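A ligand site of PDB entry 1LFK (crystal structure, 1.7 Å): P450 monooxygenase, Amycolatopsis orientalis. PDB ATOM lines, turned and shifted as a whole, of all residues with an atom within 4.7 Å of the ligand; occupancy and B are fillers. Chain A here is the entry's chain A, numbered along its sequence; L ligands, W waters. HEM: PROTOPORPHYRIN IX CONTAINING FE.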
ATOM      1  N   MET A  55      23.080  11.659  14.863  1.00  0.00           N
ATOM      2  CA  MET A  55      22.401  10.675  14.036  1.00  0.00           C
ATOM      3  C   MET A  55      20.943  10.464  14.408  1.00  0.00           C
ATOM      4  O   MET A  55      20.130  10.054  13.578  1.00  0.00           O
ATOM      5  CB  MET A  55      23.154   9.330  14.119  1.00  0.00           C
ATOM      6  CG  MET A  55      24.605   9.459  13.677  1.00  0.00           C
ATOM      7  SD  MET A  55      25.448   7.812  13.585  1.00  0.00           S
ATOM      8  CE  MET A  55      24.742   7.097  12.031  1.00  0.00           C
ATOM      9  N   LEU A  88      17.676   4.083   0.550  1.00  0.00           N
ATOM     10  CA  LEU A  88      17.275   4.622   1.845  1.00  0.00           C
ATOM     11  C   LEU A  88      18.174   5.710   2.404  1.00  0.00           C
ATOM     12  O   LEU A  88      17.656   6.650   3.027  1.00  0.00           O
ATOM     13  CB  LEU A  88      17.091   3.521   2.896  1.00  0.00           C
ATOM     14  CG  LEU A  88      16.109   2.382   2.545  1.00  0.00           C
ATOM     15  CD1 LEU A  88      15.959   1.453   3.734  1.00  0.00           C
ATOM     16  CD2 LEU A  88      14.741   2.930   2.133  1.00  0.00           C
ATOM     17  N   MET A  89      19.473   5.610   2.174  1.00  0.00           N
ATOM     18  CA  MET A  89      20.386   6.612   2.738  1.00  0.00           C
ATOM     19  C   MET A  89      20.192   8.020   2.214  1.00  0.00           C
ATOM     20  O   MET A  89      20.545   8.998   2.886  1.00  0.00           O
ATOM     21  CB  MET A  89      21.847   6.192   2.537  1.00  0.00           C
ATOM     22  CG  MET A  89      22.259   4.978   3.347  1.00  0.00           C
ATOM     23  SD  MET A  89      22.267   5.228   5.151  1.00  0.00           S
ATOM     24  CE  MET A  89      22.183   7.052   5.301  1.00  0.00           C
ATOM     25  N   HIS A  96      11.771   8.922   3.678  1.00  0.00           N
ATOM     26  CA  HIS A  96      12.573   7.781   4.052  1.00  0.00           C
ATOM     27  C   HIS A  96      11.707   6.741   4.756  1.00  0.00           C
ATOM     28  O   HIS A  96      11.845   5.534   4.527  1.00  0.00           O
ATOM     29  CB  HIS A  96      13.728   8.211   4.950  1.00  0.00           C
ATOM     30  CG  HIS A  96      14.378   7.065   5.672  1.00  0.00           C
ATOM     31  ND1 HIS A  96      13.963   6.628   6.912  1.00  0.00           N
ATOM     32  CD2 HIS A  96      15.396   6.252   5.308  1.00  0.00           C
ATOM     33  CE1 HIS A  96      14.703   5.602   7.284  1.00  0.00           C
ATOM     34  NE2 HIS A  96      15.583   5.361   6.320  1.00  0.00           N
ATOM     35  N   ARG A 100      11.405   2.865   3.672  1.00  0.00           N
ATOM     36  CA  ARG A 100      11.898   1.825   4.547  1.00  0.00           C
ATOM     37  C   ARG A 100      10.791   0.882   4.904  1.00  0.00           C
ATOM     38  O   ARG A 100      11.008  -0.323   5.047  1.00  0.00           O
ATOM     39  CB  ARG A 100      12.487   2.411   5.828  1.00  0.00           C
ATOM     40  CG  ARG A 100      13.234   1.374   6.610  1.00  0.00           C
ATOM     41  CD  ARG A 100      14.228   1.973   7.616  1.00  0.00           C
ATOM     42  NE  ARG A 100      14.564   0.997   8.650  1.00  0.00           N
ATOM     43  CZ  ARG A 100      15.786   0.797   9.115  1.00  0.00           C
ATOM     44  NH1 ARG A 100      16.806   1.469   8.627  1.00  0.00           N
ATOM     45  NH2 ARG A 100      15.986   0.003  10.156  1.00  0.00           N
ATOM     46  N   PHE A 107      13.104  -8.101   5.964  1.00  0.00           N
ATOM     47  CA  PHE A 107      14.076  -8.199   7.038  1.00  0.00           C
ATOM     48  C   PHE A 107      13.488  -8.500   8.394  1.00  0.00           C
ATOM     49  O   PHE A 107      14.164  -8.303   9.401  1.00  0.00           O
ATOM     50  CB  PHE A 107      14.884  -6.868   7.146  1.00  0.00           C
ATOM     51  CG  PHE A 107      15.758  -6.586   5.963  1.00  0.00           C
ATOM     52  CD1 PHE A 107      15.218  -6.025   4.781  1.00  0.00           C
ATOM     53  CD2 PHE A 107      17.113  -6.923   5.999  1.00  0.00           C
ATOM     54  CE1 PHE A 107      16.011  -5.797   3.656  1.00  0.00           C
ATOM     55  CE2 PHE A 107      17.937  -6.698   4.857  1.00  0.00           C
ATOM     56  CZ  PHE A 107      17.372  -6.136   3.679  1.00  0.00           C
ATOM     57  N   LEU A 152      23.863 -12.689   1.037  1.00  0.00           N
ATOM     58  CA  LEU A 152      23.031 -11.663   0.437  1.00  0.00           C
ATOM     59  C   LEU A 152      22.221 -12.252  -0.751  1.00  0.00           C
ATOM     60  O   LEU A 152      21.047 -11.931  -0.911  1.00  0.00           O
ATOM     61  CB  LEU A 152      23.876 -10.480  -0.054  1.00  0.00           C
ATOM     62  CG  LEU A 152      24.523  -9.679   1.099  1.00  0.00           C
ATOM     63  CD1 LEU A 152      25.476  -8.614   0.559  1.00  0.00           C
ATOM     64  CD2 LEU A 152      23.379  -9.032   1.937  1.00  0.00           C
ATOM     65  N   LEU A 155      19.385 -14.082   0.781  1.00  0.00           N
ATOM     66  CA  LEU A 155      18.407 -13.082   1.244  1.00  0.00           C
ATOM     67  C   LEU A 155      17.526 -12.526   0.129  1.00  0.00           C
ATOM     68  O   LEU A 155      16.297 -12.398   0.276  1.00  0.00           O
ATOM     69  CB  LEU A 155      19.141 -11.896   1.905  1.00  0.00           C
ATOM     70  CG  LEU A 155      18.275 -10.702   2.340  1.00  0.00           C
ATOM     71  CD1 LEU A 155      17.460 -11.080   3.552  1.00  0.00           C
ATOM     72  CD2 LEU A 155      19.216  -9.459   2.623  1.00  0.00           C
ATOM     73  N   GLN A 232      21.201  -1.645  -3.377  1.00  0.00           N
ATOM     74  CA  GLN A 232      21.651  -1.051  -2.109  1.00  0.00           C
ATOM     75  C   GLN A 232      22.031  -2.113  -1.110  1.00  0.00           C
ATOM     76  O   GLN A 232      22.991  -1.961  -0.395  1.00  0.00           O
ATOM     77  CB  GLN A 232      20.572  -0.275  -1.356  1.00  0.00           C
ATOM     78  CG  GLN A 232      19.831   0.843  -1.951  1.00  0.00           C
ATOM     79  CD  GLN A 232      18.615   1.157  -1.058  1.00  0.00           C
ATOM     80  OE1 GLN A 232      18.738   1.406   0.175  1.00  0.00           O
ATOM     81  NE2 GLN A 232      17.433   1.132  -1.671  1.00  0.00           N
ATOM     82  N   VAL A 233      21.211  -3.167  -1.017  1.00  0.00           N
ATOM     83  CA  VAL A 233      21.464  -4.264  -0.073  1.00  0.00           C
ATOM     84  C   VAL A 233      22.743  -5.036  -0.429  1.00  0.00           C
ATOM     85  O   VAL A 233      23.541  -5.415   0.441  1.00  0.00           O
ATOM     86  CB  VAL A 233      20.209  -5.192  -0.037  1.00  0.00           C
ATOM     87  CG1 VAL A 233      20.551  -6.529   0.633  1.00  0.00           C
ATOM     88  CG2 VAL A 233      19.084  -4.464   0.726  1.00  0.00           C
ATOM     89  N   ALA A 236      25.491  -2.787   0.705  1.00  0.00           N
ATOM     90  CA  ALA A 236      25.577  -2.513   2.129  1.00  0.00           C
ATOM     91  C   ALA A 236      25.972  -3.675   3.041  1.00  0.00           C
ATOM     92  O   ALA A 236      26.514  -3.462   4.140  1.00  0.00           O
ATOM     93  CB  ALA A 236      24.207  -1.942   2.611  1.00  0.00           C
ATOM     94  N   GLY A 237      25.761  -4.920   2.595  1.00  0.00           N
ATOM     95  CA  GLY A 237      26.017  -6.018   3.485  1.00  0.00           C
ATOM     96  C   GLY A 237      27.180  -6.910   3.133  1.00  0.00           C
ATOM     97  O   GLY A 237      27.248  -8.059   3.607  1.00  0.00           O
ATOM     98  N   ASN A 240      31.233  -4.844   5.023  1.00  0.00           N
ATOM     99  CA  ASN A 240      31.219  -4.762   6.496  1.00  0.00           C
ATOM    100  C   ASN A 240      31.299  -6.148   7.095  1.00  0.00           C
ATOM    101  O   ASN A 240      31.936  -6.336   8.117  1.00  0.00           O
ATOM    102  CB  ASN A 240      29.926  -4.110   6.992  1.00  0.00           C
ATOM    103  CG  ASN A 240      29.840  -2.605   6.767  1.00  0.00           C
ATOM    104  OD1 ASN A 240      30.836  -1.874   6.813  1.00  0.00           O
ATOM    105  ND2 ASN A 240      28.624  -2.133   6.560  1.00  0.00           N
ATOM    106  N   ILE A 241      30.644  -7.117   6.451  1.00  0.00           N
ATOM    107  CA  ILE A 241      30.661  -8.463   6.990  1.00  0.00           C
ATOM    108  C   ILE A 241      31.995  -9.130   6.714  1.00  0.00           C
ATOM    109  O   ILE A 241      32.508  -9.776   7.588  1.00  0.00           O
ATOM    110  CB  ILE A 241      29.503  -9.345   6.390  1.00  0.00           C
ATOM    111  CG1 ILE A 241      28.134  -8.750   6.796  1.00  0.00           C
ATOM    112  CG2 ILE A 241      29.700 -10.822   6.847  1.00  0.00           C
ATOM    113  CD1 ILE A 241      27.731  -8.957   8.265  1.00  0.00           C
ATOM    114  N   MET A 244      34.369  -7.867   9.193  1.00  0.00           N
ATOM    115  CA  MET A 244      34.118  -8.438  10.503  1.00  0.00           C
ATOM    116  C   MET A 244      34.555  -9.881  10.658  1.00  0.00           C
ATOM    117  O   MET A 244      34.962 -10.280  11.724  1.00  0.00           O
ATOM    118  CB  MET A 244      32.616  -8.308  10.900  1.00  0.00           C
ATOM    119  CG  MET A 244      32.237  -6.937  11.454  1.00  0.00           C
ATOM    120  SD  MET A 244      33.168  -6.536  12.947  1.00  0.00           S
ATOM    121  CE  MET A 244      32.855  -7.938  14.122  1.00  0.00           C
ATOM    122  N   ILE A 277      31.620  -6.556  17.310  1.00  0.00           N
ATOM    123  CA  ILE A 277      31.140  -5.496  16.430  1.00  0.00           C
ATOM    124  C   ILE A 277      31.502  -4.124  17.055  1.00  0.00           C
ATOM    125  O   ILE A 277      32.019  -3.228  16.358  1.00  0.00           O
ATOM    126  CB  ILE A 277      29.598  -5.608  16.214  1.00  0.00           C
ATOM    127  CG1 ILE A 277      29.340  -6.803  15.275  1.00  0.00           C
ATOM    128  CG2 ILE A 277      29.020  -4.284  15.623  1.00  0.00           C
ATOM    129  CD1 ILE A 277      27.834  -7.133  15.129  1.00  0.00           C
ATOM    130  N   VAL A 282      33.886  -1.718  12.157  1.00  0.00           N
ATOM    131  CA  VAL A 282      34.501  -1.657  10.823  1.00  0.00           C
ATOM    132  C   VAL A 282      34.176  -0.420   9.988  1.00  0.00           C
ATOM    133  O   VAL A 282      35.073   0.031   9.272  1.00  0.00           O
ATOM    134  CB  VAL A 282      34.291  -2.990  10.011  1.00  0.00           C
ATOM    135  CG1 VAL A 282      34.912  -4.147  10.793  1.00  0.00           C
ATOM    136  CG2 VAL A 282      32.808  -3.241   9.736  1.00  0.00           C
ATOM    137  N   PRO A 283      32.948   0.150  10.030  1.00  0.00           N
ATOM    138  CA  PRO A 283      32.704   1.340   9.217  1.00  0.00           C
ATOM    139  C   PRO A 283      33.447   2.533   9.834  1.00  0.00           C
ATOM    140  O   PRO A 283      33.349   2.738  11.047  1.00  0.00           O
ATOM    141  CB  PRO A 283      31.184   1.596   9.330  1.00  0.00           C
ATOM    142  CG  PRO A 283      30.607   0.286   9.902  1.00  0.00           C
ATOM    143  CD  PRO A 283      31.728  -0.270  10.768  1.00  0.00           C
ATOM    144  N   PRO A 286      29.265   6.858   9.259  1.00  0.00           N
ATOM    145  CA  PRO A 286      27.973   6.659   8.621  1.00  0.00           C
ATOM    146  C   PRO A 286      27.937   7.735   7.524  1.00  0.00           C
ATOM    147  O   PRO A 286      28.928   8.401   7.261  1.00  0.00           O
ATOM    148  CB  PRO A 286      26.988   6.986   9.703  1.00  0.00           C
ATOM    149  CG  PRO A 286      27.684   8.114  10.451  1.00  0.00           C
ATOM    150  CD  PRO A 286      29.124   7.644  10.511  1.00  0.00           C
ATOM    151  N   THR A 287      26.785   7.921   6.889  1.00  0.00           N
ATOM    152  CA  THR A 287      26.661   8.943   5.845  1.00  0.00           C
ATOM    153  C   THR A 287      26.854  10.304   6.525  1.00  0.00           C
ATOM    154  O   THR A 287      26.380  10.511   7.620  1.00  0.00           O
ATOM    155  CB  THR A 287      25.252   8.899   5.269  1.00  0.00           C
ATOM    156  OG1 THR A 287      24.995   7.557   4.793  1.00  0.00           O
ATOM    157  CG2 THR A 287      25.107   9.891   4.085  1.00  0.00           C
ATOM    158  N   ARG A 289      26.220  13.973   7.789  1.00  0.00           N
ATOM    159  CA  ARG A 289      24.964  14.621   8.137  1.00  0.00           C
ATOM    160  C   ARG A 289      25.134  16.136   7.906  1.00  0.00           C
ATOM    161  O   ARG A 289      26.208  16.716   8.135  1.00  0.00           O
ATOM    162  CB  ARG A 289      24.614  14.365   9.616  1.00  0.00           C
ATOM    163  CG  ARG A 289      24.545  12.839   9.961  1.00  0.00           C
ATOM    164  CD  ARG A 289      23.530  12.177   9.100  1.00  0.00           C
ATOM    165  NE  ARG A 289      22.770  11.087   9.728  1.00  0.00           N
ATOM    166  CZ  ARG A 289      23.000   9.786   9.504  1.00  0.00           C
ATOM    167  NH1 ARG A 289      23.970   9.414   8.717  1.00  0.00           N
ATOM    168  NH2 ARG A 289      22.200   8.887  10.025  1.00  0.00           N
ATOM    169  N   LEU A 312      32.402   6.538  14.059  1.00  0.00           N
ATOM    170  CA  LEU A 312      31.830   5.436  14.851  1.00  0.00           C
ATOM    171  C   LEU A 312      32.910   4.702  15.640  1.00  0.00           C
ATOM    172  O   LEU A 312      32.690   4.309  16.768  1.00  0.00           O
ATOM    173  CB  LEU A 312      31.074   4.473  13.927  1.00  0.00           C
ATOM    174  CG  LEU A 312      30.055   5.171  13.015  1.00  0.00           C
ATOM    175  CD1 LEU A 312      29.336   4.141  12.256  1.00  0.00           C
ATOM    176  CD2 LEU A 312      28.982   5.936  13.829  1.00  0.00           C
ATOM    177  N   ALA A 339      27.953   1.094  16.125  1.00  0.00           N
ATOM    178  CA  ALA A 339      28.504   0.534  14.889  1.00  0.00           C
ATOM    179  C   ALA A 339      27.449   0.273  13.805  1.00  0.00           C
ATOM    180  O   ALA A 339      27.798   0.216  12.602  1.00  0.00           O
ATOM    181  CB  ALA A 339      29.308  -0.755  15.186  1.00  0.00           C
ATOM    182  N   PHE A 340      26.168   0.105  14.193  1.00  0.00           N
ATOM    183  CA  PHE A 340      25.107  -0.069  13.202  1.00  0.00           C
ATOM    184  C   PHE A 340      24.355   1.254  13.075  1.00  0.00           C
ATOM    185  O   PHE A 340      23.264   1.316  12.515  1.00  0.00           O
ATOM    186  CB  PHE A 340      24.091  -1.143  13.641  1.00  0.00           C
ATOM    187  CG  PHE A 340      24.585  -2.561  13.556  1.00  0.00           C
ATOM    188  CD1 PHE A 340      24.600  -3.381  14.687  1.00  0.00           C
ATOM    189  CD2 PHE A 340      24.937  -3.094  12.339  1.00  0.00           C
ATOM    190  CE1 PHE A 340      24.969  -4.772  14.625  1.00  0.00           C
ATOM    191  CE2 PHE A 340      25.316  -4.464  12.231  1.00  0.00           C
ATOM    192  CZ  PHE A 340      25.326  -5.278  13.350  1.00  0.00           C
ATOM    193  N   GLY A 341      24.940   2.340  13.594  1.00  0.00           N
ATOM    194  CA  GLY A 341      24.259   3.629  13.484  1.00  0.00           C
ATOM    195  C   GLY A 341      23.306   3.876  14.650  1.00  0.00           C
ATOM    196  O   GLY A 341      23.372   3.239  15.719  1.00  0.00           O
ATOM    197  N   VAL A 344      16.562   6.687  12.849  1.00  0.00           N
ATOM    198  CA  VAL A 344      15.752   6.092  11.805  1.00  0.00           C
ATOM    199  C   VAL A 344      16.528   5.328  10.705  1.00  0.00           C
ATOM    200  O   VAL A 344      15.940   4.439  10.072  1.00  0.00           O
ATOM    201  CB  VAL A 344      14.790   7.146  11.146  1.00  0.00           C
ATOM    202  CG1 VAL A 344      13.821   7.696  12.237  1.00  0.00           C
ATOM    203  CG2 VAL A 344      15.564   8.274  10.486  1.00  0.00           C
ATOM    204  N   HIS A 345      17.804   5.658  10.470  1.00  0.00           N
ATOM    205  CA  HIS A 345      18.611   4.959   9.461  1.00  0.00           C
ATOM    206  C   HIS A 345      19.411   3.779  10.032  1.00  0.00           C
ATOM    207  O   HIS A 345      20.224   3.189   9.301  1.00  0.00           O
ATOM    208  CB  HIS A 345      19.596   5.907   8.775  1.00  0.00           C
ATOM    209  CG  HIS A 345      18.949   6.917   7.878  1.00  0.00           C
ATOM    210  ND1 HIS A 345      18.579   6.642   6.587  1.00  0.00           N
ATOM    211  CD2 HIS A 345      18.607   8.213   8.105  1.00  0.00           C
ATOM    212  CE1 HIS A 345      18.027   7.722   6.042  1.00  0.00           C
ATOM    213  NE2 HIS A 345      18.039   8.686   6.948  1.00  0.00           N
ATOM    214  N   HIS A 346      19.179   3.443  11.295  1.00  0.00           N
ATOM    215  CA  HIS A 346      19.886   2.326  11.984  1.00  0.00           C
ATOM    216  C   HIS A 346      19.892   1.100  11.052  1.00  0.00           C
ATOM    217  O   HIS A 346      18.854   0.754  10.459  1.00  0.00           O
ATOM    218  CB  HIS A 346      19.195   1.996  13.327  1.00  0.00           C
ATOM    219  CG  HIS A 346      19.802   0.847  14.069  1.00  0.00           C
ATOM    220  ND1 HIS A 346      19.362  -0.460  13.881  1.00  0.00           N
ATOM    221  CD2 HIS A 346      20.827   0.775  14.957  1.00  0.00           C
ATOM    222  CE1 HIS A 346      20.094  -1.275  14.619  1.00  0.00           C
ATOM    223  NE2 HIS A 346      20.993  -0.559  15.272  1.00  0.00           N
ATOM    224  N   CYS A 347      21.072   0.451  10.913  1.00  0.00           N
ATOM    225  CA  CYS A 347      21.270  -0.653   9.957  1.00  0.00           C
ATOM    226  C   CYS A 347      20.058  -1.580   9.784  1.00  0.00           C
ATOM    227  O   CYS A 347      19.633  -2.255  10.750  1.00  0.00           O
ATOM    228  CB  CYS A 347      22.492  -1.476  10.385  1.00  0.00           C
ATOM    229  SG  CYS A 347      22.813  -2.747   9.120  1.00  0.00           S
ATOM    230  N   LEU A 348      19.474  -1.567   8.579  1.00  0.00           N
ATOM    231  CA  LEU A 348      18.315  -2.418   8.260  1.00  0.00           C
ATOM    232  C   LEU A 348      18.694  -3.917   8.332  1.00  0.00           C
ATOM    233  O   LEU A 348      17.890  -4.759   8.762  1.00  0.00           O
ATOM    234  CB  LEU A 348      17.795  -2.041   6.873  1.00  0.00           C
ATOM    235  CG  LEU A 348      16.520  -2.785   6.455  1.00  0.00           C
ATOM    236  CD1 LEU A 348      15.370  -2.506   7.402  1.00  0.00           C
ATOM    237  CD2 LEU A 348      16.178  -2.383   5.015  1.00  0.00           C
ATOM    238  N   GLY A 349      19.967  -4.215   8.067  1.00  0.00           N
ATOM    239  CA  GLY A 349      20.394  -5.610   8.121  1.00  0.00           C
ATOM    240  C   GLY A 349      21.077  -6.010   9.424  1.00  0.00           C
ATOM    241  O   GLY A 349      21.789  -7.015   9.477  1.00  0.00           O
ATOM    242  N   LEU A 352      20.401  -9.628  10.554  1.00  0.00           N
ATOM    243  CA  LEU A 352      21.054 -10.567   9.599  1.00  0.00           C
ATOM    244  C   LEU A 352      22.560 -10.611   9.864  1.00  0.00           C
ATOM    245  O   LEU A 352      23.199 -11.673   9.868  1.00  0.00           O
ATOM    246  CB  LEU A 352      20.806 -10.148   8.145  1.00  0.00           C
ATOM    247  CG  LEU A 352      21.411 -11.099   7.105  1.00  0.00           C
ATOM    248  CD1 LEU A 352      21.015 -12.539   7.381  1.00  0.00           C
ATOM    249  CD2 LEU A 352      20.905 -10.717   5.756  1.00  0.00           C
ATOM    250  N   ALA A 353      23.151  -9.446  10.031  1.00  0.00           N
ATOM    251  CA  ALA A 353      24.580  -9.360  10.300  1.00  0.00           C
ATOM    252  C   ALA A 353      24.975 -10.135  11.560  1.00  0.00           C
ATOM    253  O   ALA A 353      25.993 -10.873  11.564  1.00  0.00           O
ATOM    254  CB  ALA A 353      25.013  -7.847  10.475  1.00  0.00           C
ATOM    255  N   LEU A 357      27.229 -13.497  11.494  1.00  0.00           N
ATOM    256  CA  LEU A 357      28.530 -13.526  12.143  1.00  0.00           C
ATOM    257  C   LEU A 357      28.584 -14.611  13.227  1.00  0.00           C
ATOM    258  O   LEU A 357      29.562 -15.321  13.358  1.00  0.00           O
ATOM    259  CB  LEU A 357      28.842 -12.124  12.730  1.00  0.00           C
ATOM    260  CG  LEU A 357      29.198 -11.090  11.630  1.00  0.00           C
ATOM    261  CD1 LEU A 357      29.395  -9.670  12.318  1.00  0.00           C
ATOM    262  CD2 LEU A 357      30.535 -11.452  10.979  1.00  0.00           C
HETATM  263  CHA HEM L   1      22.690   1.199   7.294  1.00  0.00           C
HETATM  264  CHB HEM L   1      26.553  -0.647   9.558  1.00  0.00           C
HETATM  265  CHC HEM L   1      25.600  -5.010   7.663  1.00  0.00           C
HETATM  266  CHD HEM L   1      21.969  -3.071   5.154  1.00  0.00           C
HETATM  267  C1A HEM L   1      23.805   1.080   8.114  1.00  0.00           C
HETATM  268  C2A HEM L   1      24.343   2.149   8.923  1.00  0.00           C
HETATM  269  C3A HEM L   1      25.475   1.645   9.499  1.00  0.00           C
HETATM  270  C4A HEM L   1      25.588   0.258   9.090  1.00  0.00           C
HETATM  271  CMA HEM L   1      26.467   2.413  10.395  1.00  0.00           C
HETATM  272  CAA HEM L   1      23.731   3.531   9.171  1.00  0.00           C
HETATM  273  CBA HEM L   1      24.296   4.528   8.171  1.00  0.00           C
HETATM  274  CGA HEM L   1      23.829   5.939   8.437  1.00  0.00           C
HETATM  275  O1A HEM L   1      24.278   6.851   7.696  1.00  0.00           O
HETATM  276  O2A HEM L   1      23.031   6.153   9.373  1.00  0.00           O
HETATM  277  C1B HEM L   1      26.638  -2.010   9.251  1.00  0.00           C
HETATM  278  C2B HEM L   1      27.583  -2.946   9.834  1.00  0.00           C
HETATM  279  C3B HEM L   1      27.321  -4.182   9.306  1.00  0.00           C
HETATM  280  C4B HEM L   1      26.199  -3.983   8.397  1.00  0.00           C
HETATM  281  CMB HEM L   1      28.634  -2.610  10.895  1.00  0.00           C
HETATM  282  CAB HEM L   1      27.978  -5.391   9.550  1.00  0.00           C
HETATM  283  CBB HEM L   1      28.453  -5.860  10.764  1.00  0.00           C
HETATM  284  C1C HEM L   1      24.500  -4.878   6.832  1.00  0.00           C
HETATM  285  C2C HEM L   1      23.868  -5.961   6.108  1.00  0.00           C
HETATM  286  C3C HEM L   1      22.867  -5.415   5.365  1.00  0.00           C
HETATM  287  C4C HEM L   1      22.861  -3.991   5.661  1.00  0.00           C
HETATM  288  CMC HEM L   1      24.302  -7.436   6.155  1.00  0.00           C
HETATM  289  CAC HEM L   1      22.023  -6.022   4.418  1.00  0.00           C
HETATM  290  CBC HEM L   1      21.447  -7.262   4.533  1.00  0.00           C
HETATM  291  C1D HEM L   1      21.881  -1.715   5.469  1.00  0.00           C
HETATM  292  C2D HEM L   1      20.927  -0.792   4.883  1.00  0.00           C
HETATM  293  C3D HEM L   1      21.096   0.401   5.541  1.00  0.00           C
HETATM  294  C4D HEM L   1      22.171   0.201   6.482  1.00  0.00           C
HETATM  295  CMD HEM L   1      19.915  -1.100   3.781  1.00  0.00           C
HETATM  296  CAD HEM L   1      20.335   1.709   5.317  1.00  0.00           C
HETATM  297  CBD HEM L   1      19.116   1.802   6.222  1.00  0.00           C
HETATM  298  CGD HEM L   1      18.439   3.172   6.163  1.00  0.00           C
HETATM  299  O1D HEM L   1      17.313   3.287   6.681  1.00  0.00           O
HETATM  300  O2D HEM L   1      19.041   4.119   5.610  1.00  0.00           O
HETATM  301  NA  HEM L   1      24.545  -0.078   8.247  1.00  0.00           N
HETATM  302  NB  HEM L   1      25.774  -2.658   8.396  1.00  0.00           N
HETATM  303  NC  HEM L   1      23.852  -3.679   6.570  1.00  0.00           N
HETATM  304  ND  HEM L   1      22.659  -1.096   6.438  1.00  0.00           N
HETATM  305 FE   HEM L   1      24.141  -1.883   7.461  1.00  0.00          FE
HETATM  306  O   HOH W   1      21.847   5.234  11.627  1.00  0.00           O
HETATM  307  O   HOH W   2      27.728   1.072   6.537  1.00  0.00           O
HETATM  308  O   HOH W   3      25.695  -1.339   5.926  1.00  0.00           O
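NH1 of Arg 100 is in hydrogen-bond range of O of Val 344 (3.4 Å).
The side-chain sulfur (SG) of Cys 347 sits close to the backbone NH (N) of Gly 349.
A ring nitrogen (NE2) of His 96 lies within hydrogen-bond range of a ring nitrogen (ND1) of His 345 (3.3 Å).
ND2 of Asn 240 sits at hydrogen-bond distance from O of Ala 236, at 3.5 Å.
N of Leu 88 sits at hydrogen-bond distance from OE1 of Gln 232 (2.9 Å).
The backbone carbonyl oxygen of His 346 is in hydrogen-bond range of the guanidinium group of Arg 100 (2.8 Å).
N of Cys 347 sits at hydrogen-bond distance from O of Phe 340 (2.8 Å).
OG1 of Thr 287 sits close to SD of Met 89 (3.6 Å).
SD of Met 89 lies close to O2D of the ligand.
The side-chain amide nitrogen (ND2) of Asn 240 lies close to a nitrogen (NB) of the ligand.
Met 55 touches the ligand (CE to O2A, 3.3 Å).
CB of Leu 88 touches O2D of the ligand (3.4 Å).
CE2 of Phe 107 touches CBC of the ligand, 3.6 Å away.
Leu 152 touches the ligand.
Leu 155 touches the ligand.
CB of Ala 236 touches CHD of the ligand (3.6 Å).
Gly 237 touches the ligand (CA to C2C, 3.4 Å).
Ile 241 touches the ligand.
Met 244 touches the ligand.
Pro 283 touches the ligand.
CB of Pro 286 touches O1A of the ligand, at 3.4 Å.
Leu 312 touches the ligand (CD1 to CMA, 3.8 Å).
Ala 339 touches the ligand.
CE2 of Phe 340 touches C3B of the ligand, 3.6 Å away.
Gly 341 touches the ligand (N to CMA, 3.5 Å).
Val 344 touches the ligand (O to O1D, 3.8 Å).
Leu 348 touches the ligand (N to C4D, 3.8 Å).
Gly 349 touches the ligand.
Leu 352 touches the ligand.
CB of Ala 353 touches CAB of the ligand, 3.96 Å away.
Hydrophobic or aromatic side chains that line the ligand: Met 55, Leu 88, Met 89, His 96, Phe 107, Leu 152, Leu 155, Ala 236, Ile 241, Met 244, Pro 283, Pro 286, Leu 312, Phe 340, His 345, Leu 348, Leu 352 and Ala 353.
The nearest printed residue that does not touch the ligand is Val 233 (4.1 Å).
O1D of the ligand lies within hydrogen-bond range of NE2 of His 96 (2.7 Å).
An oxygen (O1A) of the ligand is in salt-bridge range of the guanidinium group of Arg 289.
An oxygen (O1A) of the ligand is in hydrogen-bond range of the backbone NH (N) of Thr 287, 2.8 Å away.
The guanidinium group (NH1) of Arg 100 is in salt-bridge range of an oxygen (O1D) of the ligand (2.7 Å).
FE of the ligand is bound by SG of Cys 347, 2.3 Å away.
ND1 of His 345 sits at hydrogen-bond distance from O2D of the ligand (2.7 Å).
O1A of the ligand lies within hydrogen-bond range of OG1 of Thr 287, at 3.1 Å.
Water W3 bridges the backbone carbonyl oxygen (O) of Ala 236 (2.9 Å) and the side-chain amide nitrogen (ND2) of Asn 240 (3.1 Å).
Water W1 lies within hydrogen-bond range of O2A of the ligand, N of His 346 and O of His 345.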
